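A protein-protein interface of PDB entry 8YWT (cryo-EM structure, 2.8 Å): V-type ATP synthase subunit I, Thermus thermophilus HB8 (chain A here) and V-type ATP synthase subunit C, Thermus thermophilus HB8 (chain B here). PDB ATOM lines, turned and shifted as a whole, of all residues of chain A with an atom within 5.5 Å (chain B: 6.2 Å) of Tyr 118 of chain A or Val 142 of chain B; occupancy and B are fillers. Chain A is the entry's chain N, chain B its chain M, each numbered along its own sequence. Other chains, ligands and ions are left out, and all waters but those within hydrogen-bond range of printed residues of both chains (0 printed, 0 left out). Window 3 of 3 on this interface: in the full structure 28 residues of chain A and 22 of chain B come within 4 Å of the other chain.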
ATOM      1  N   LEU A 114     -19.745 -19.765 -15.630  1.00  0.00           N
ATOM      2  CA  LEU A 114     -18.860 -18.701 -16.099  1.00  0.00           C
ATOM      3  C   LEU A 114     -18.045 -18.087 -14.955  1.00  0.00           C
ATOM      4  O   LEU A 114     -16.855 -17.825 -15.119  1.00  0.00           O
ATOM      5  CB  LEU A 114     -19.702 -17.656 -16.846  1.00  0.00           C
ATOM      6  CG  LEU A 114     -18.872 -16.644 -17.657  1.00  0.00           C
ATOM      7  CD1 LEU A 114     -18.106 -17.303 -18.807  1.00  0.00           C
ATOM      8  CD2 LEU A 114     -19.805 -15.609 -18.272  1.00  0.00           C
ATOM      9  N   ALA A 115     -18.654 -17.903 -13.780  1.00  0.00           N
ATOM     10  CA  ALA A 115     -17.970 -17.363 -12.611  1.00  0.00           C
ATOM     11  C   ALA A 115     -16.825 -18.273 -12.154  1.00  0.00           C
ATOM     12  O   ALA A 115     -15.700 -17.803 -12.011  1.00  0.00           O
ATOM     13  CB  ALA A 115     -18.987 -17.131 -11.490  1.00  0.00           C
ATOM     14  N   GLN A 116     -17.062 -19.577 -11.984  1.00  0.00           N
ATOM     15  CA  GLN A 116     -16.017 -20.492 -11.509  1.00  0.00           C
ATOM     16  C   GLN A 116     -14.849 -20.684 -12.499  1.00  0.00           C
ATOM     17  O   GLN A 116     -13.756 -21.053 -12.077  1.00  0.00           O
ATOM     18  CB  GLN A 116     -16.641 -21.820 -11.046  1.00  0.00           C
ATOM     19  CG  GLN A 116     -17.100 -22.762 -12.171  1.00  0.00           C
ATOM     20  CD  GLN A 116     -17.756 -24.050 -11.668  1.00  0.00           C
ATOM     21  OE1 GLN A 116     -17.891 -24.315 -10.482  1.00  0.00           O
ATOM     22  NE2 GLN A 116     -18.171 -24.922 -12.555  1.00  0.00           N
ATOM     23  N   ALA A 117     -15.027 -20.399 -13.792  1.00  0.00           N
ATOM     24  CA  ALA A 117     -13.943 -20.363 -14.774  1.00  0.00           C
ATOM     25  C   ALA A 117     -13.053 -19.117 -14.616  1.00  0.00           C
ATOM     26  O   ALA A 117     -11.835 -19.235 -14.489  1.00  0.00           O
ATOM     27  CB  ALA A 117     -14.548 -20.423 -16.181  1.00  0.00           C
ATOM     28  N   TYR A 118     -13.650 -17.922 -14.581  1.00  0.00           N
ATOM     29  CA  TYR A 118     -12.922 -16.661 -14.409  1.00  0.00           C
ATOM     30  C   TYR A 118     -12.326 -16.469 -13.003  1.00  0.00           C
ATOM     31  O   TYR A 118     -11.384 -15.693 -12.846  1.00  0.00           O
ATOM     32  CB  TYR A 118     -13.864 -15.495 -14.711  1.00  0.00           C
ATOM     33  CG  TYR A 118     -13.883 -15.019 -16.142  1.00  0.00           C
ATOM     34  CD1 TYR A 118     -12.985 -14.010 -16.537  1.00  0.00           C
ATOM     35  CD2 TYR A 118     -14.857 -15.485 -17.042  1.00  0.00           C
ATOM     36  CE1 TYR A 118     -13.105 -13.414 -17.805  1.00  0.00           C
ATOM     37  CE2 TYR A 118     -14.967 -14.902 -18.319  1.00  0.00           C
ATOM     38  CZ  TYR A 118     -14.121 -13.840 -18.684  1.00  0.00           C
ATOM     39  OH  TYR A 118     -14.321 -13.176 -19.849  1.00  0.00           O
ATOM     40  N   LEU A 119     -12.853 -17.143 -11.979  1.00  0.00           N
ATOM     41  CA  LEU A 119     -12.458 -16.925 -10.587  1.00  0.00           C
ATOM     42  C   LEU A 119     -10.961 -17.151 -10.331  1.00  0.00           C
ATOM     43  O   LEU A 119     -10.341 -16.324  -9.672  1.00  0.00           O
ATOM     44  CB  LEU A 119     -13.342 -17.801  -9.681  1.00  0.00           C
ATOM     45  CG  LEU A 119     -13.074 -17.661  -8.174  1.00  0.00           C
ATOM     46  CD1 LEU A 119     -13.276 -16.229  -7.681  1.00  0.00           C
ATOM     47  CD2 LEU A 119     -14.053 -18.552  -7.409  1.00  0.00           C
ATOM     48  N   GLU A 120     -10.355 -18.216 -10.866  1.00  0.00           N
ATOM     49  CA  GLU A 120      -8.919 -18.459 -10.679  1.00  0.00           C
ATOM     50  C   GLU A 120      -8.039 -17.333 -11.251  1.00  0.00           C
ATOM     51  O   GLU A 120      -7.305 -16.733 -10.466  1.00  0.00           O
ATOM     52  CB  GLU A 120      -8.482 -19.850 -11.173  1.00  0.00           C
ATOM     53  CG  GLU A 120      -6.963 -20.018 -10.984  1.00  0.00           C
ATOM     54  CD  GLU A 120      -6.385 -21.388 -11.354  1.00  0.00           C
ATOM     55  OE1 GLU A 120      -5.184 -21.593 -11.073  1.00  0.00           O
ATOM     56  OE2 GLU A 120      -7.095 -22.239 -11.923  1.00  0.00           O
ATOM     57  N   PRO A 121      -8.058 -16.997 -12.558  1.00  0.00           N
ATOM     58  CA  PRO A 121      -7.255 -15.889 -13.059  1.00  0.00           C
ATOM     59  C   PRO A 121      -7.574 -14.561 -12.356  1.00  0.00           C
ATOM     60  O   PRO A 121      -6.643 -13.826 -12.049  1.00  0.00           O
ATOM     61  CB  PRO A 121      -7.482 -15.838 -14.571  1.00  0.00           C
ATOM     62  CG  PRO A 121      -8.769 -16.626 -14.792  1.00  0.00           C
ATOM     63  CD  PRO A 121      -8.758 -17.642 -13.655  1.00  0.00           C
ATOM     64  N   LEU A 122      -8.825 -14.252 -11.989  1.00  0.00           N
ATOM     65  CA  LEU A 122      -9.094 -13.036 -11.209  1.00  0.00           C
ATOM     66  C   LEU A 122      -8.438 -13.063  -9.819  1.00  0.00           C
ATOM     67  O   LEU A 122      -7.865 -12.058  -9.412  1.00  0.00           O
ATOM     68  CB  LEU A 122     -10.606 -12.766 -11.106  1.00  0.00           C
ATOM     69  CG  LEU A 122     -11.057 -11.672 -12.086  1.00  0.00           C
ATOM     70  CD1 LEU A 122     -12.579 -11.666 -12.187  1.00  0.00           C
ATOM     71  CD2 LEU A 122     -10.615 -10.283 -11.618  1.00  0.00           C
ATOM     72  N   GLU A 123      -8.451 -14.184  -9.101  1.00  0.00           N
ATOM     73  CA  GLU A 123      -7.725 -14.302  -7.830  1.00  0.00           C
ATOM     74  C   GLU A 123      -6.200 -14.234  -8.015  1.00  0.00           C
ATOM     75  O   GLU A 123      -5.522 -13.572  -7.230  1.00  0.00           O
ATOM     76  CB  GLU A 123      -8.116 -15.591  -7.093  1.00  0.00           C
ATOM     77  CG  GLU A 123      -9.503 -15.481  -6.445  1.00  0.00           C
ATOM     78  CD  GLU A 123      -9.819 -16.674  -5.526  1.00  0.00           C
ATOM     79  OE1 GLU A 123      -9.415 -17.822  -5.825  1.00  0.00           O
ATOM     80  OE2 GLU A 123     -10.452 -16.461  -4.468  1.00  0.00           O
ATOM     81  N   LEU A 144      -3.906 -12.198 -20.030  1.00  0.00           N
ATOM     82  CA  LEU A 144      -3.429 -13.585 -20.000  1.00  0.00           C
ATOM     83  C   LEU A 144      -2.535 -13.873 -21.212  1.00  0.00           C
ATOM     84  O   LEU A 144      -2.818 -13.403 -22.316  1.00  0.00           O
ATOM     85  CB  LEU A 144      -4.627 -14.552 -19.957  1.00  0.00           C
ATOM     86  CG  LEU A 144      -5.588 -14.342 -18.777  1.00  0.00           C
ATOM     87  CD1 LEU A 144      -6.753 -15.324 -18.863  1.00  0.00           C
ATOM     88  CD2 LEU A 144      -4.895 -14.512 -17.427  1.00  0.00           C
ATOM     89  N   TYR A 172       0.653 -20.314 -14.257  1.00  0.00           N
ATOM     90  CA  TYR A 172      -0.310 -21.308 -13.771  1.00  0.00           C
ATOM     91  C   TYR A 172      -0.566 -22.347 -14.885  1.00  0.00           C
ATOM     92  O   TYR A 172       0.011 -22.235 -15.968  1.00  0.00           O
ATOM     93  CB  TYR A 172      -1.577 -20.606 -13.252  1.00  0.00           C
ATOM     94  CG  TYR A 172      -2.436 -19.927 -14.301  1.00  0.00           C
ATOM     95  CD1 TYR A 172      -2.118 -18.635 -14.768  1.00  0.00           C
ATOM     96  CD2 TYR A 172      -3.579 -20.584 -14.791  1.00  0.00           C
ATOM     97  CE1 TYR A 172      -2.925 -18.023 -15.745  1.00  0.00           C
ATOM     98  CE2 TYR A 172      -4.386 -19.972 -15.765  1.00  0.00           C
ATOM     99  CZ  TYR A 172      -4.052 -18.694 -16.255  1.00  0.00           C
ATOM    100  OH  TYR A 172      -4.811 -18.111 -17.214  1.00  0.00           O
ATOM    101  N   LEU A 202      -7.968  -8.225 -20.416  1.00  0.00           N
ATOM    102  CA  LEU A 202      -8.921  -9.279 -20.061  1.00  0.00           C
ATOM    103  C   LEU A 202     -10.279  -8.678 -19.657  1.00  0.00           C
ATOM    104  O   LEU A 202     -10.404  -8.072 -18.595  1.00  0.00           O
ATOM    105  CB  LEU A 202      -8.329 -10.164 -18.946  1.00  0.00           C
ATOM    106  CG  LEU A 202      -9.262 -11.303 -18.490  1.00  0.00           C
ATOM    107  CD1 LEU A 202      -9.469 -12.344 -19.585  1.00  0.00           C
ATOM    108  CD2 LEU A 202      -8.696 -12.003 -17.261  1.00  0.00           C
ATOM    109  N   ARG A 203     -11.315  -8.882 -20.479  1.00  0.00           N
ATOM    110  CA  ARG A 203     -12.698  -8.473 -20.176  1.00  0.00           C
ATOM    111  C   ARG A 203     -13.315  -9.405 -19.124  1.00  0.00           C
ATOM    112  O   ARG A 203     -13.636 -10.556 -19.427  1.00  0.00           O
ATOM    113  CB  ARG A 203     -13.534  -8.465 -21.473  1.00  0.00           C
ATOM    114  CG  ARG A 203     -13.070  -7.449 -22.535  1.00  0.00           C
ATOM    115  CD  ARG A 203     -13.167  -5.976 -22.105  1.00  0.00           C
ATOM    116  NE  ARG A 203     -14.555  -5.570 -21.796  1.00  0.00           N
ATOM    117  CZ  ARG A 203     -15.478  -5.122 -22.630  1.00  0.00           C
ATOM    118  NH1 ARG A 203     -16.658  -4.816 -22.191  1.00  0.00           N
ATOM    119  NH2 ARG A 203     -15.264  -4.959 -23.900  1.00  0.00           N
ATOM    120  N   LEU A 204     -13.477  -8.911 -17.894  1.00  0.00           N
ATOM    121  CA  LEU A 204     -14.209  -9.609 -16.825  1.00  0.00           C
ATOM    122  C   LEU A 204     -15.698  -9.719 -17.213  1.00  0.00           C
ATOM    123  O   LEU A 204     -16.192  -8.840 -17.920  1.00  0.00           O
ATOM    124  CB  LEU A 204     -14.017  -8.905 -15.465  1.00  0.00           C
ATOM    125  CG  LEU A 204     -12.575  -8.722 -14.941  1.00  0.00           C
ATOM    126  CD1 LEU A 204     -11.639  -9.873 -15.316  1.00  0.00           C
ATOM    127  CD2 LEU A 204     -11.951  -7.395 -15.367  1.00  0.00           C
ATOM    128  N   PRO A 205     -16.419 -10.783 -16.822  1.00  0.00           N
ATOM    129  CA  PRO A 205     -17.585 -11.230 -17.583  1.00  0.00           C
ATOM    130  C   PRO A 205     -18.762 -10.238 -17.608  1.00  0.00           C
ATOM    131  O   PRO A 205     -19.177  -9.788 -18.677  1.00  0.00           O
ATOM    132  CB  PRO A 205     -17.956 -12.606 -17.011  1.00  0.00           C
ATOM    133  CG  PRO A 205     -17.272 -12.653 -15.645  1.00  0.00           C
ATOM    134  CD  PRO A 205     -16.029 -11.795 -15.856  1.00  0.00           C
ATOM    135  N   LEU A 220     -17.143 -12.491  -8.011  1.00  0.00           N
ATOM    136  CA  LEU A 220     -17.124 -13.862  -8.535  1.00  0.00           C
ATOM    137  C   LEU A 220     -17.044 -14.870  -7.390  1.00  0.00           C
ATOM    138  O   LEU A 220     -17.778 -15.855  -7.411  1.00  0.00           O
ATOM    139  CB  LEU A 220     -15.975 -14.082  -9.529  1.00  0.00           C
ATOM    140  CG  LEU A 220     -16.283 -13.567 -10.941  1.00  0.00           C
ATOM    141  CD1 LEU A 220     -16.250 -12.046 -11.035  1.00  0.00           C
ATOM    142  CD2 LEU A 220     -15.251 -14.138 -11.899  1.00  0.00           C
ATOM    143  N   GLN B 126     -19.839 -14.586 -24.247  1.00  0.00           N
ATOM    144  CA  GLN B 126     -18.910 -13.705 -23.550  1.00  0.00           C
ATOM    145  C   GLN B 126     -17.778 -13.203 -24.464  1.00  0.00           C
ATOM    146  O   GLN B 126     -17.423 -12.026 -24.421  1.00  0.00           O
ATOM    147  CB  GLN B 126     -18.347 -14.453 -22.332  1.00  0.00           C
ATOM    148  CG  GLN B 126     -17.441 -13.576 -21.470  1.00  0.00           C
ATOM    149  CD  GLN B 126     -18.207 -12.377 -20.936  1.00  0.00           C
ATOM    150  OE1 GLN B 126     -19.008 -12.494 -20.023  1.00  0.00           O
ATOM    151  NE2 GLN B 126     -18.034 -11.205 -21.507  1.00  0.00           N
ATOM    152  N   ALA B 137      -9.579 -13.430 -28.310  1.00  0.00           N
ATOM    153  CA  ALA B 137      -8.447 -14.272 -27.920  1.00  0.00           C
ATOM    154  C   ALA B 137      -8.227 -14.338 -26.400  1.00  0.00           C
ATOM    155  O   ALA B 137      -7.867 -15.391 -25.888  1.00  0.00           O
ATOM    156  CB  ALA B 137      -7.189 -13.759 -28.618  1.00  0.00           C
ATOM    157  N   GLN B 138      -8.477 -13.255 -25.658  1.00  0.00           N
ATOM    158  CA  GLN B 138      -8.387 -13.254 -24.195  1.00  0.00           C
ATOM    159  C   GLN B 138      -9.497 -14.075 -23.543  1.00  0.00           C
ATOM    160  O   GLN B 138      -9.218 -14.834 -22.619  1.00  0.00           O
ATOM    161  CB  GLN B 138      -8.417 -11.819 -23.649  1.00  0.00           C
ATOM    162  CG  GLN B 138      -7.119 -11.055 -23.915  1.00  0.00           C
ATOM    163  CD  GLN B 138      -5.942 -11.617 -23.132  1.00  0.00           C
ATOM    164  OE1 GLN B 138      -5.965 -11.709 -21.915  1.00  0.00           O
ATOM    165  NE2 GLN B 138      -4.888 -12.040 -23.793  1.00  0.00           N
ATOM    166  N   VAL B 139     -10.746 -13.982 -24.010  1.00  0.00           N
ATOM    167  CA  VAL B 139     -11.834 -14.764 -23.392  1.00  0.00           C
ATOM    168  C   VAL B 139     -11.638 -16.259 -23.646  1.00  0.00           C
ATOM    169  O   VAL B 139     -11.885 -17.067 -22.767  1.00  0.00           O
ATOM    170  CB  VAL B 139     -13.230 -14.282 -23.817  1.00  0.00           C
ATOM    171  CG1 VAL B 139     -14.335 -15.098 -23.140  1.00  0.00           C
ATOM    172  CG2 VAL B 139     -13.449 -12.816 -23.439  1.00  0.00           C
ATOM    173  N   LEU B 140     -11.095 -16.658 -24.795  1.00  0.00           N
ATOM    174  CA  LEU B 140     -10.709 -18.050 -25.036  1.00  0.00           C
ATOM    175  C   LEU B 140      -9.464 -18.510 -24.257  1.00  0.00           C
ATOM    176  O   LEU B 140      -9.206 -19.709 -24.190  1.00  0.00           O
ATOM    177  CB  LEU B 140     -10.538 -18.264 -26.545  1.00  0.00           C
ATOM    178  CG  LEU B 140     -11.804 -18.017 -27.369  1.00  0.00           C
ATOM    179  CD1 LEU B 140     -11.511 -18.366 -28.817  1.00  0.00           C
ATOM    180  CD2 LEU B 140     -12.975 -18.875 -26.921  1.00  0.00           C
ATOM    181  N   ALA B 141      -8.704 -17.606 -23.634  1.00  0.00           N
ATOM    182  CA  ALA B 141      -7.546 -17.958 -22.816  1.00  0.00           C
ATOM    183  C   ALA B 141      -7.923 -18.414 -21.394  1.00  0.00           C
ATOM    184  O   ALA B 141      -7.224 -19.252 -20.834  1.00  0.00           O
ATOM    185  CB  ALA B 141      -6.579 -16.776 -22.784  1.00  0.00           C
ATOM    186  N   VAL B 142      -9.028 -17.939 -20.812  1.00  0.00           N
ATOM    187  CA  VAL B 142      -9.490 -18.378 -19.477  1.00  0.00           C
ATOM    188  C   VAL B 142      -9.961 -19.844 -19.443  1.00  0.00           C
ATOM    189  O   VAL B 142      -9.622 -20.540 -18.487  1.00  0.00           O
ATOM    190  CB  VAL B 142     -10.434 -17.370 -18.767  1.00  0.00           C
ATOM    191  CG1 VAL B 142     -10.913 -16.194 -19.613  1.00  0.00           C
ATOM    192  CG2 VAL B 142     -11.660 -17.987 -18.096  1.00  0.00           C
ATOM    193  N   PRO B 143     -10.627 -20.392 -20.478  1.00  0.00           N
ATOM    194  CA  PRO B 143     -10.810 -21.835 -20.636  1.00  0.00           C
ATOM    195  C   PRO B 143      -9.507 -22.618 -20.867  1.00  0.00           C
ATOM    196  O   PRO B 143      -9.464 -23.821 -20.620  1.00  0.00           O
ATOM    197  CB  PRO B 143     -11.731 -21.992 -21.855  1.00  0.00           C
ATOM    198  CG  PRO B 143     -12.494 -20.680 -21.919  1.00  0.00           C
ATOM    199  CD  PRO B 143     -11.454 -19.685 -21.436  1.00  0.00           C
ATOM    200  N   GLY B 144      -8.460 -21.960 -21.375  1.00  0.00           N
ATOM    201  CA  GLY B 144      -7.216 -22.585 -21.824  1.00  0.00           C
ATOM    202  C   GLY B 144      -7.302 -23.213 -23.219  1.00  0.00           C
ATOM    203  O   GLY B 144      -6.647 -24.215 -23.487  1.00  0.00           O
ATOM    204  N   HIS B 145      -8.136 -22.677 -24.107  1.00  0.00           N
ATOM    205  CA  HIS B 145      -8.454 -23.299 -25.393  1.00  0.00           C
ATOM    206  C   HIS B 145      -7.343 -23.081 -26.448  1.00  0.00           C
ATOM    207  O   HIS B 145      -6.867 -21.952 -26.589  1.00  0.00           O
ATOM    208  CB  HIS B 145      -9.809 -22.752 -25.845  1.00  0.00           C
ATOM    209  CG  HIS B 145     -10.311 -23.410 -27.090  1.00  0.00           C
ATOM    210  ND1 HIS B 145     -10.778 -24.691 -27.220  1.00  0.00           N
ATOM    211  CD2 HIS B 145     -10.271 -22.873 -28.336  1.00  0.00           C
ATOM    212  CE1 HIS B 145     -11.018 -24.913 -28.518  1.00  0.00           C
ATOM    213  NE2 HIS B 145     -10.696 -23.837 -29.243  1.00  0.00           N
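N of Leu 144 of chain A sits at hydrogen-bond distance from OE1 of Gln 138 of chain B, at 2.8 Å.
The backbone carbonyl oxygen of Pro 205 of chain A lies close to the side-chain amide oxygen of Gln 126 of chain B (3.0 Å).
The backbone carbonyl oxygen of Arg 203 of chain A sits at hydrogen-bond distance from the side-chain hydroxyl of Tyr 118 of chain A (2.7 Å).
Gln 126 of chain B touches Leu 114 of chain A.
Val 142 of chain B touches Ala 117 of chain A.
Tyr 118 of chain A touches Gln 126 of chain B.
Val 139 of chain B touches Tyr 118 of chain A.
CE1 of Tyr 118 of chain A touches CG1 of Val 142 of chain B (3.98 Å).
Val 142 of chain B touches Leu 144 of chain A (N to CD1, 3.98 Å).
Leu 202 of chain A touches Gln 138 of chain B.
Printed residues of chain B that touch a printed residue of chain A: Gln 126, Gln 138, Val 139 and Val 142.
Printed residues of chain A that touch a printed residue of chain B: Leu 114, Ala 117, Tyr 118, Leu 144, Leu 202 and Pro 205.
Hydrophobic or aromatic side chains of chain A within 4 Å of the printed part of chain B: Leu 114, Tyr 118, Leu 144, Leu 202 and Pro 205.
Among the printed residues, 9 pairs touch across the chains.
Tyr 118 of chain A touches three residues of chain B.
Val 142 of chain B touches three residues of chain A.
Of the printed residues of chain B, Leu 144 of chain A touches Gln 138 and Val 142.
Printed residues of chain B within 4 Å of Pro 205 of chain A: Gln 126.
Of the printed residues of chain B, Leu 202 of chain A touches Gln 138 (3.9 Å).
His 145 of chain B touches none of the printed residues of chain A.
Glu 123 of chain A touches none of the printed residues of chain B.
The nearest residue of chain B that does not touch Tyr 118 of chain A is Gln 138 of chain B (6.0 Å).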
